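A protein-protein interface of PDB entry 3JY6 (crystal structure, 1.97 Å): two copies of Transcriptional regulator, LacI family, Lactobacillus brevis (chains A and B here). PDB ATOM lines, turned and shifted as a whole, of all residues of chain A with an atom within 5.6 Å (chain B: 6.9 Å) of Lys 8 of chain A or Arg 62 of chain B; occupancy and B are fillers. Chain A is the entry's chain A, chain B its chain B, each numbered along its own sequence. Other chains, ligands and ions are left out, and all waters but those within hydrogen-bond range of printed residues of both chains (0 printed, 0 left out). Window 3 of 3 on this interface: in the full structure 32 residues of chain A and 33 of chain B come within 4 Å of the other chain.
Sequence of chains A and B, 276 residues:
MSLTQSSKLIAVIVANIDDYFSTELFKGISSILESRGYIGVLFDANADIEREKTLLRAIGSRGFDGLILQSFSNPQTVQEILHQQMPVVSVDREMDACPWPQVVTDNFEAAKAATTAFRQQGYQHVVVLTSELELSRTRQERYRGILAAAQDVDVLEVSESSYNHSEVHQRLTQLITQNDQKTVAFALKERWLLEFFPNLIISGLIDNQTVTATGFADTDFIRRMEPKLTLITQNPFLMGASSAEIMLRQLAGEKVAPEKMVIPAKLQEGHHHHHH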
ATOM      1  N   SER A   6      23.641 -26.966  -9.065  1.00  0.00           N
ATOM      2  CA  SER A   6      23.996 -26.750 -10.470  1.00  0.00           C
ATOM      3  C   SER A   6      22.707 -26.557 -11.281  1.00  0.00           C
ATOM      4  O   SER A   6      21.621 -26.459 -10.705  1.00  0.00           O
ATOM      5  CB  SER A   6      24.788 -27.946 -11.018  1.00  0.00           C
ATOM      6  OG  SER A   6      24.009 -29.133 -11.018  1.00  0.00           O
ATOM      7  N   SER A   7      22.819 -26.502 -12.608  1.00  0.00           N
ATOM      8  CA  SER A   7      21.633 -26.303 -13.454  1.00  0.00           C
ATOM      9  C   SER A   7      20.670 -27.484 -13.408  1.00  0.00           C
ATOM     10  O   SER A   7      19.458 -27.291 -13.399  1.00  0.00           O
ATOM     11  CB  SER A   7      22.039 -26.035 -14.915  1.00  0.00           C
ATOM     12  OG  SER A   7      22.409 -27.228 -15.597  1.00  0.00           O
ATOM     13  N   LYS A   8      21.218 -28.699 -13.378  1.00  0.00           N
ATOM     14  CA  LYS A   8      20.436 -29.942 -13.340  1.00  0.00           C
ATOM     15  C   LYS A   8      19.620 -30.122 -14.625  1.00  0.00           C
ATOM     16  O   LYS A   8      18.617 -30.839 -14.653  1.00  0.00           O
ATOM     17  CB  LYS A   8      19.520 -29.980 -12.111  1.00  0.00           C
ATOM     18  CG  LYS A   8      20.201 -29.516 -10.824  1.00  0.00           C
ATOM     19  CD  LYS A   8      19.524 -30.052  -9.571  1.00  0.00           C
ATOM     20  CE  LYS A   8      19.684 -31.563  -9.472  1.00  0.00           C
ATOM     21  NZ  LYS A   8      19.049 -32.150  -8.254  1.00  0.00           N
ATOM     22  N   LEU A   9      20.075 -29.456 -15.682  1.00  0.00           N
ATOM     23  CA  LEU A   9      19.447 -29.538 -16.990  1.00  0.00           C
ATOM     24  C   LEU A   9      20.264 -30.485 -17.853  1.00  0.00           C
ATOM     25  O   LEU A   9      21.488 -30.344 -17.962  1.00  0.00           O
ATOM     26  CB  LEU A   9      19.428 -28.173 -17.680  1.00  0.00           C
ATOM     27  CG  LEU A   9      18.512 -27.080 -17.155  1.00  0.00           C
ATOM     28  CD1 LEU A   9      18.538 -25.901 -18.125  1.00  0.00           C
ATOM     29  CD2 LEU A   9      17.112 -27.634 -17.003  1.00  0.00           C
ATOM     30  N   ILE A  10      19.581 -31.445 -18.460  1.00  0.00           N
ATOM     31  CA  ILE A  10      20.220 -32.409 -19.346  1.00  0.00           C
ATOM     32  C   ILE A  10      19.747 -32.111 -20.761  1.00  0.00           C
ATOM     33  O   ILE A  10      18.544 -32.087 -21.032  1.00  0.00           O
ATOM     34  CB  ILE A  10      19.836 -33.860 -18.977  1.00  0.00           C
ATOM     35  CG1 ILE A  10      20.267 -34.152 -17.539  1.00  0.00           C
ATOM     36  CG2 ILE A  10      20.504 -34.852 -19.945  1.00  0.00           C
ATOM     37  CD1 ILE A  10      21.767 -33.957 -17.287  1.00  0.00           C
ATOM     38  N   ARG A  36      15.045 -37.777 -10.018  1.00  0.00           N
ATOM     39  CA  ARG A  36      16.190 -37.236  -9.303  1.00  0.00           C
ATOM     40  C   ARG A  36      16.380 -35.724  -9.418  1.00  0.00           C
ATOM     41  O   ARG A  36      17.466 -35.207  -9.161  1.00  0.00           O
ATOM     42  CB  ARG A  36      17.464 -37.972  -9.732  1.00  0.00           C
ATOM     43  CG  ARG A  36      17.396 -39.468  -9.459  1.00  0.00           C
ATOM     44  CD  ARG A  36      18.761 -40.124  -9.564  1.00  0.00           C
ATOM     45  NE  ARG A  36      18.678 -41.586  -9.501  1.00  0.00           N
ATOM     46  CZ  ARG A  36      19.730 -42.392  -9.635  1.00  0.00           C
ATOM     47  NH1 ARG A  36      20.937 -41.879  -9.838  1.00  0.00           N
ATOM     48  NH2 ARG A  36      19.577 -43.711  -9.576  1.00  0.00           N
ATOM     49  N   GLY A  37      15.321 -35.010  -9.794  1.00  0.00           N
ATOM     50  CA  GLY A  37      15.411 -33.560  -9.886  1.00  0.00           C
ATOM     51  C   GLY A  37      16.018 -33.001 -11.151  1.00  0.00           C
ATOM     52  O   GLY A  37      16.180 -31.788 -11.290  1.00  0.00           O
ATOM     53  N   TYR A  38      16.369 -33.876 -12.082  1.00  0.00           N
ATOM     54  CA  TYR A  38      16.950 -33.427 -13.331  1.00  0.00           C
ATOM     55  C   TYR A  38      15.835 -33.144 -14.337  1.00  0.00           C
ATOM     56  O   TYR A  38      14.745 -33.724 -14.271  1.00  0.00           O
ATOM     57  CB  TYR A  38      17.935 -34.484 -13.844  1.00  0.00           C
ATOM     58  CG  TYR A  38      19.263 -34.449 -13.105  1.00  0.00           C
ATOM     59  CD1 TYR A  38      20.262 -33.532 -13.463  1.00  0.00           C
ATOM     60  CD2 TYR A  38      19.501 -35.285 -12.017  1.00  0.00           C
ATOM     61  CE1 TYR A  38      21.471 -33.451 -12.750  1.00  0.00           C
ATOM     62  CE2 TYR A  38      20.705 -35.209 -11.295  1.00  0.00           C
ATOM     63  CZ  TYR A  38      21.683 -34.284 -11.670  1.00  0.00           C
ATOM     64  OH  TYR A  38      22.860 -34.169 -10.950  1.00  0.00           O
ATOM     65  N   ILE A  39      16.104 -32.236 -15.260  1.00  0.00           N
ATOM     66  CA  ILE A  39      15.108 -31.876 -16.248  1.00  0.00           C
ATOM     67  C   ILE A  39      15.619 -32.014 -17.668  1.00  0.00           C
ATOM     68  O   ILE A  39      16.606 -31.382 -18.038  1.00  0.00           O
ATOM     69  CB  ILE A  39      14.641 -30.437 -16.025  1.00  0.00           C
ATOM     70  CG1 ILE A  39      14.059 -30.324 -14.622  1.00  0.00           C
ATOM     71  CG2 ILE A  39      13.596 -30.051 -17.067  1.00  0.00           C
ATOM     72  CD1 ILE A  39      13.696 -28.933 -14.247  1.00  0.00           C
ATOM     73  N   ARG A  62      26.156 -22.652 -21.698  1.00  0.00           N
ATOM     74  CA  ARG A  62      24.985 -22.277 -20.908  1.00  0.00           C
ATOM     75  C   ARG A  62      24.937 -23.148 -19.656  1.00  0.00           C
ATOM     76  O   ARG A  62      24.070 -22.986 -18.791  1.00  0.00           O
ATOM     77  CB  ARG A  62      23.704 -22.464 -21.724  1.00  0.00           C
ATOM     78  CG  ARG A  62      23.198 -21.195 -22.393  1.00  0.00           C
ATOM     79  CD  ARG A  62      22.563 -20.265 -21.364  1.00  0.00           C
ATOM     80  NE  ARG A  62      21.914 -19.116 -21.981  1.00  0.00           N
ATOM     81  CZ  ARG A  62      21.054 -18.319 -21.356  1.00  0.00           C
ATOM     82  NH1 ARG A  62      20.732 -18.543 -20.087  1.00  0.00           N
ATOM     83  NH2 ARG A  62      20.519 -17.293 -22.000  1.00  0.00           N
ATOM     84  N   ASP A  65      24.107 -30.039 -17.597  1.00  0.00           N
ATOM     85  CA  ASP A  65      24.895 -31.041 -16.893  1.00  0.00           C
ATOM     86  C   ASP A  65      25.090 -32.368 -17.598  1.00  0.00           C
ATOM     87  O   ASP A  65      25.757 -33.254 -17.066  1.00  0.00           O
ATOM     88  CB  ASP A  65      24.324 -31.290 -15.499  1.00  0.00           C
ATOM     89  CG  ASP A  65      24.405 -30.055 -14.606  1.00  0.00           C
ATOM     90  OD1 ASP A  65      25.168 -29.114 -14.925  1.00  0.00           O
ATOM     91  OD2 ASP A  65      23.709 -30.029 -13.570  1.00  0.00           O
ATOM     92  N   THR B  54       6.273 -27.506 -12.388  1.00  0.00           N
ATOM     93  CA  THR B  54       7.666 -27.727 -12.036  1.00  0.00           C
ATOM     94  C   THR B  54       8.581 -27.271 -13.174  1.00  0.00           C
ATOM     95  O   THR B  54       9.681 -26.766 -12.928  1.00  0.00           O
ATOM     96  CB  THR B  54       7.943 -29.213 -11.627  1.00  0.00           C
ATOM     97  OG1 THR B  54       9.335 -29.509 -11.796  1.00  0.00           O
ATOM     98  CG2 THR B  54       7.116 -30.176 -12.432  1.00  0.00           C
ATOM     99  N   LEU B  55       8.118 -27.410 -14.418  1.00  0.00           N
ATOM    100  CA  LEU B  55       8.899 -26.961 -15.571  1.00  0.00           C
ATOM    101  C   LEU B  55       8.968 -25.439 -15.536  1.00  0.00           C
ATOM    102  O   LEU B  55      10.019 -24.853 -15.766  1.00  0.00           O
ATOM    103  CB  LEU B  55       8.244 -27.390 -16.893  1.00  0.00           C
ATOM    104  CG  LEU B  55       8.268 -28.860 -17.306  1.00  0.00           C
ATOM    105  CD1 LEU B  55       7.462 -29.023 -18.574  1.00  0.00           C
ATOM    106  CD2 LEU B  55       9.713 -29.333 -17.516  1.00  0.00           C
ATOM    107  N   ARG B  57       8.875 -23.505 -13.040  1.00  0.00           N
ATOM    108  CA  ARG B  57       9.800 -23.038 -12.009  1.00  0.00           C
ATOM    109  C   ARG B  57      11.236 -23.127 -12.519  1.00  0.00           C
ATOM    110  O   ARG B  57      12.021 -22.187 -12.364  1.00  0.00           O
ATOM    111  CB  ARG B  57       9.642 -23.852 -10.721  1.00  0.00           C
ATOM    112  CG  ARG B  57       8.418 -23.465  -9.912  1.00  0.00           C
ATOM    113  CD  ARG B  57       8.621 -23.742  -8.430  1.00  0.00           C
ATOM    114  NE  ARG B  57       7.954 -22.735  -7.608  1.00  0.00           N
ATOM    115  CZ  ARG B  57       8.323 -21.458  -7.546  1.00  0.00           C
ATOM    116  NH1 ARG B  57       9.357 -21.023  -8.255  1.00  0.00           N
ATOM    117  NH2 ARG B  57       7.660 -20.616  -6.769  1.00  0.00           N
ATOM    118  N   ALA B  58      11.567 -24.254 -13.143  1.00  0.00           N
ATOM    119  CA  ALA B  58      12.903 -24.461 -13.693  1.00  0.00           C
ATOM    120  C   ALA B  58      13.229 -23.417 -14.749  1.00  0.00           C
ATOM    121  O   ALA B  58      14.330 -22.861 -14.765  1.00  0.00           O
ATOM    122  CB  ALA B  58      13.009 -25.838 -14.297  1.00  0.00           C
ATOM    123  N   ILE B  59      12.279 -23.165 -15.644  1.00  0.00           N
ATOM    124  CA  ILE B  59      12.467 -22.171 -16.696  1.00  0.00           C
ATOM    125  C   ILE B  59      12.767 -20.815 -16.051  1.00  0.00           C
ATOM    126  O   ILE B  59      13.645 -20.078 -16.492  1.00  0.00           O
ATOM    127  CB  ILE B  59      11.185 -22.061 -17.591  1.00  0.00           C
ATOM    128  CG1 ILE B  59      11.249 -23.076 -18.737  1.00  0.00           C
ATOM    129  CG2 ILE B  59      11.045 -20.670 -18.159  1.00  0.00           C
ATOM    130  CD1 ILE B  59      11.326 -24.507 -18.307  1.00  0.00           C
ATOM    131  N   GLY B  60      12.038 -20.504 -14.988  1.00  0.00           N
ATOM    132  CA  GLY B  60      12.219 -19.227 -14.322  1.00  0.00           C
ATOM    133  C   GLY B  60      13.519 -19.047 -13.560  1.00  0.00           C
ATOM    134  O   GLY B  60      14.189 -18.024 -13.698  1.00  0.00           O
ATOM    135  N   SER B  61      13.881 -20.037 -12.754  1.00  0.00           N
ATOM    136  CA  SER B  61      15.094 -19.946 -11.967  1.00  0.00           C
ATOM    137  C   SER B  61      16.390 -20.169 -12.741  1.00  0.00           C
ATOM    138  O   SER B  61      17.451 -19.738 -12.294  1.00  0.00           O
ATOM    139  CB  SER B  61      15.024 -20.937 -10.813  1.00  0.00           C
ATOM    140  OG  SER B  61      14.861 -22.245 -11.315  1.00  0.00           O
ATOM    141  N   ARG B  62      16.321 -20.841 -13.888  1.00  0.00           N
ATOM    142  CA  ARG B  62      17.530 -21.109 -14.671  1.00  0.00           C
ATOM    143  C   ARG B  62      17.963 -19.937 -15.563  1.00  0.00           C
ATOM    144  O   ARG B  62      19.023 -19.978 -16.194  1.00  0.00           O
ATOM    145  CB  ARG B  62      17.348 -22.388 -15.499  1.00  0.00           C
ATOM    146  CG  ARG B  62      17.746 -23.685 -14.771  1.00  0.00           C
ATOM    147  CD  ARG B  62      16.922 -23.913 -13.504  1.00  0.00           C
ATOM    148  NE  ARG B  62      17.394 -25.032 -12.684  1.00  0.00           N
ATOM    149  CZ  ARG B  62      16.882 -26.263 -12.702  1.00  0.00           C
ATOM    150  NH1 ARG B  62      15.869 -26.556 -13.505  1.00  0.00           N
ATOM    151  NH2 ARG B  62      17.373 -27.201 -11.899  1.00  0.00           N
ATOM    152  N   GLY B  63      17.141 -18.895 -15.618  1.00  0.00           N
ATOM    153  CA  GLY B  63      17.496 -17.728 -16.404  1.00  0.00           C
ATOM    154  C   GLY B  63      17.205 -17.748 -17.892  1.00  0.00           C
ATOM    155  O   GLY B  63      17.861 -17.042 -18.659  1.00  0.00           O
ATOM    156  N   PHE B  64      16.239 -18.553 -18.316  1.00  0.00           N
ATOM    157  CA  PHE B  64      15.877 -18.589 -19.726  1.00  0.00           C
ATOM    158  C   PHE B  64      15.423 -17.178 -20.058  1.00  0.00           C
ATOM    159  O   PHE B  64      14.883 -16.484 -19.197  1.00  0.00           O
ATOM    160  CB  PHE B  64      14.744 -19.594 -19.964  1.00  0.00           C
ATOM    161  CG  PHE B  64      15.189 -21.027 -19.906  1.00  0.00           C
ATOM    162  CD1 PHE B  64      15.482 -21.635 -18.687  1.00  0.00           C
ATOM    163  CD2 PHE B  64      15.344 -21.764 -21.078  1.00  0.00           C
ATOM    164  CE1 PHE B  64      15.923 -22.958 -18.638  1.00  0.00           C
ATOM    165  CE2 PHE B  64      15.788 -23.089 -21.043  1.00  0.00           C
ATOM    166  CZ  PHE B  64      16.077 -23.688 -19.822  1.00  0.00           C
ATOM    167  N   GLN B  85       9.434 -11.925 -14.824  1.00  0.00           N
ATOM    168  CA  GLN B  85      10.870 -11.871 -15.015  1.00  0.00           C
ATOM    169  C   GLN B  85      11.283 -12.081 -16.483  1.00  0.00           C
ATOM    170  O   GLN B  85      12.447 -11.879 -16.834  1.00  0.00           O
ATOM    171  CB  GLN B  85      11.560 -12.890 -14.102  1.00  0.00           C
ATOM    172  CG  GLN B  85      11.277 -14.341 -14.421  1.00  0.00           C
ATOM    173  CD  GLN B  85      11.828 -15.269 -13.358  1.00  0.00           C
ATOM    174  OE1 GLN B  85      11.169 -15.555 -12.359  1.00  0.00           O
ATOM    175  NE2 GLN B  85      13.055 -15.730 -13.559  1.00  0.00           N
ATOM    176  N   MET B  86      10.335 -12.461 -17.341  1.00  0.00           N
ATOM    177  CA  MET B  86      10.649 -12.676 -18.755  1.00  0.00           C
ATOM    178  C   MET B  86       9.458 -12.484 -19.699  1.00  0.00           C
ATOM    179  O   MET B  86       8.308 -12.526 -19.279  1.00  0.00           O
ATOM    180  CB  MET B  86      11.243 -14.085 -18.975  1.00  0.00           C
ATOM    181  CG  MET B  86      10.276 -15.271 -18.756  1.00  0.00           C
ATOM    182  SD  MET B  86      11.058 -16.943 -18.942  1.00  0.00           S
ATOM    183  CE  MET B  86      11.763 -17.115 -17.281  1.00  0.00           C
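The backbone carbonyl oxygen (O) of Ser 7 of chain A lies within hydrogen-bond range of the guanidinium group (NH2) of Arg 62 of chain B (2.6 Å).
N of Ile 10 of chain A is in hydrogen-bond range of O of Ile 39 of chain A (3.0 Å).
The backbone carbonyl oxygen (O) of Lys 8 of chain A sits at hydrogen-bond distance from the backbone NH (N) of Ile 39 of chain A (2.9 Å).
The backbone NH (N) of Asp 65 of chain A sits at hydrogen-bond distance from the backbone carbonyl oxygen (O) of Leu 9 of chain A (2.7 Å).
The side-chain hydroxyl of Ser 7 of chain A is in hydrogen-bond range of the side-chain carboxylate of Asp 65 of chain A (3.4 Å).
OD2 of Asp 65 of chain A lies within hydrogen-bond range of N of Lys 8 of chain A (2.8 Å).
The backbone NH (N) of Leu 9 of chain A sits close to the side-chain hydroxyl (OG) of Ser 7 of chain A (3.2 Å).
Lys 8 of chain A touches Arg 62 of chain B.
Leu 9 of chain A touches Arg 62 of chain B (CD2 to NH1, 3.9 Å).
CZ of Phe 64 of chain B touches CD1 of Leu 9 of chain A (3.7 Å).
Ile 39 of chain A touches Leu 55 of chain B (CG2 to CD2, 3.97 Å).
CD1 of Ile 39 of chain A touches CB of Ala 58 of chain B (3.2 Å).
Ile 39 of chain A touches Arg 62 of chain B.
NH1 of Arg 62 of chain A touches O of Gly 63 of chain B, at 3.5 Å.
Printed residues of chain B within 4 Å of Ser 7 of chain A: Arg 62 (2.6 Å).
Of the printed residues of chain B, Lys 8 of chain A touches Arg 62.
Printed residues of chain B within 4 Å of Ile 39 of chain A: Leu 55 (3.97 Å), Ala 58 (3.2 Å) and Arg 62 (3.3 Å).
Of the printed residues of chain A, Ala 58 of chain B touches Ile 39.
Arg 62 of chain B touches just these residues of chain A: Ser 7 (2.6 Å), Lys 8 (3.5 Å), Leu 9 (3.9 Å) and Ile 39 (3.3 Å).
Printed residues of chain A within 4 Å of Gly 63 of chain B: Arg 62.
The nearest printed residue of chain A that does not touch Arg 62 of chain B is Ser 6 of chain A (4.5 Å).
The nearest printed residue of chain A that does not touch Leu 55 of chain B is Tyr 38 of chain A (7.4 Å).
Of the 12 printed residues of chain B, 5 touch a printed residue of chain A.
Printed residues of chain B that touch a printed residue of chain A: Leu 55, Ala 58, Arg 62, Gly 63 and Phe 64.
Hydrophobic or aromatic side chains of chain B within 4 Å of the printed part of chain A: Leu 55, Ala 58 and Phe 64.
Of the 11 printed residues of chain A, 5 touch a printed residue of chain B.
Hydrophobic or aromatic side chains of chain A that line the printed part of chain B: Leu 9 and Ile 39.
Among the printed residues, 8 pairs touch across the chains.
Among the printed residues, no Asp or Glu carboxylate lies within 4 Å of a Lys or Arg side-chain nitrogen of the other chain.
Position printed for both chains: 62.
Of the 8 pairs that touch across the chains among the printed residues, none has its exchanged pair printed and touching as well.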
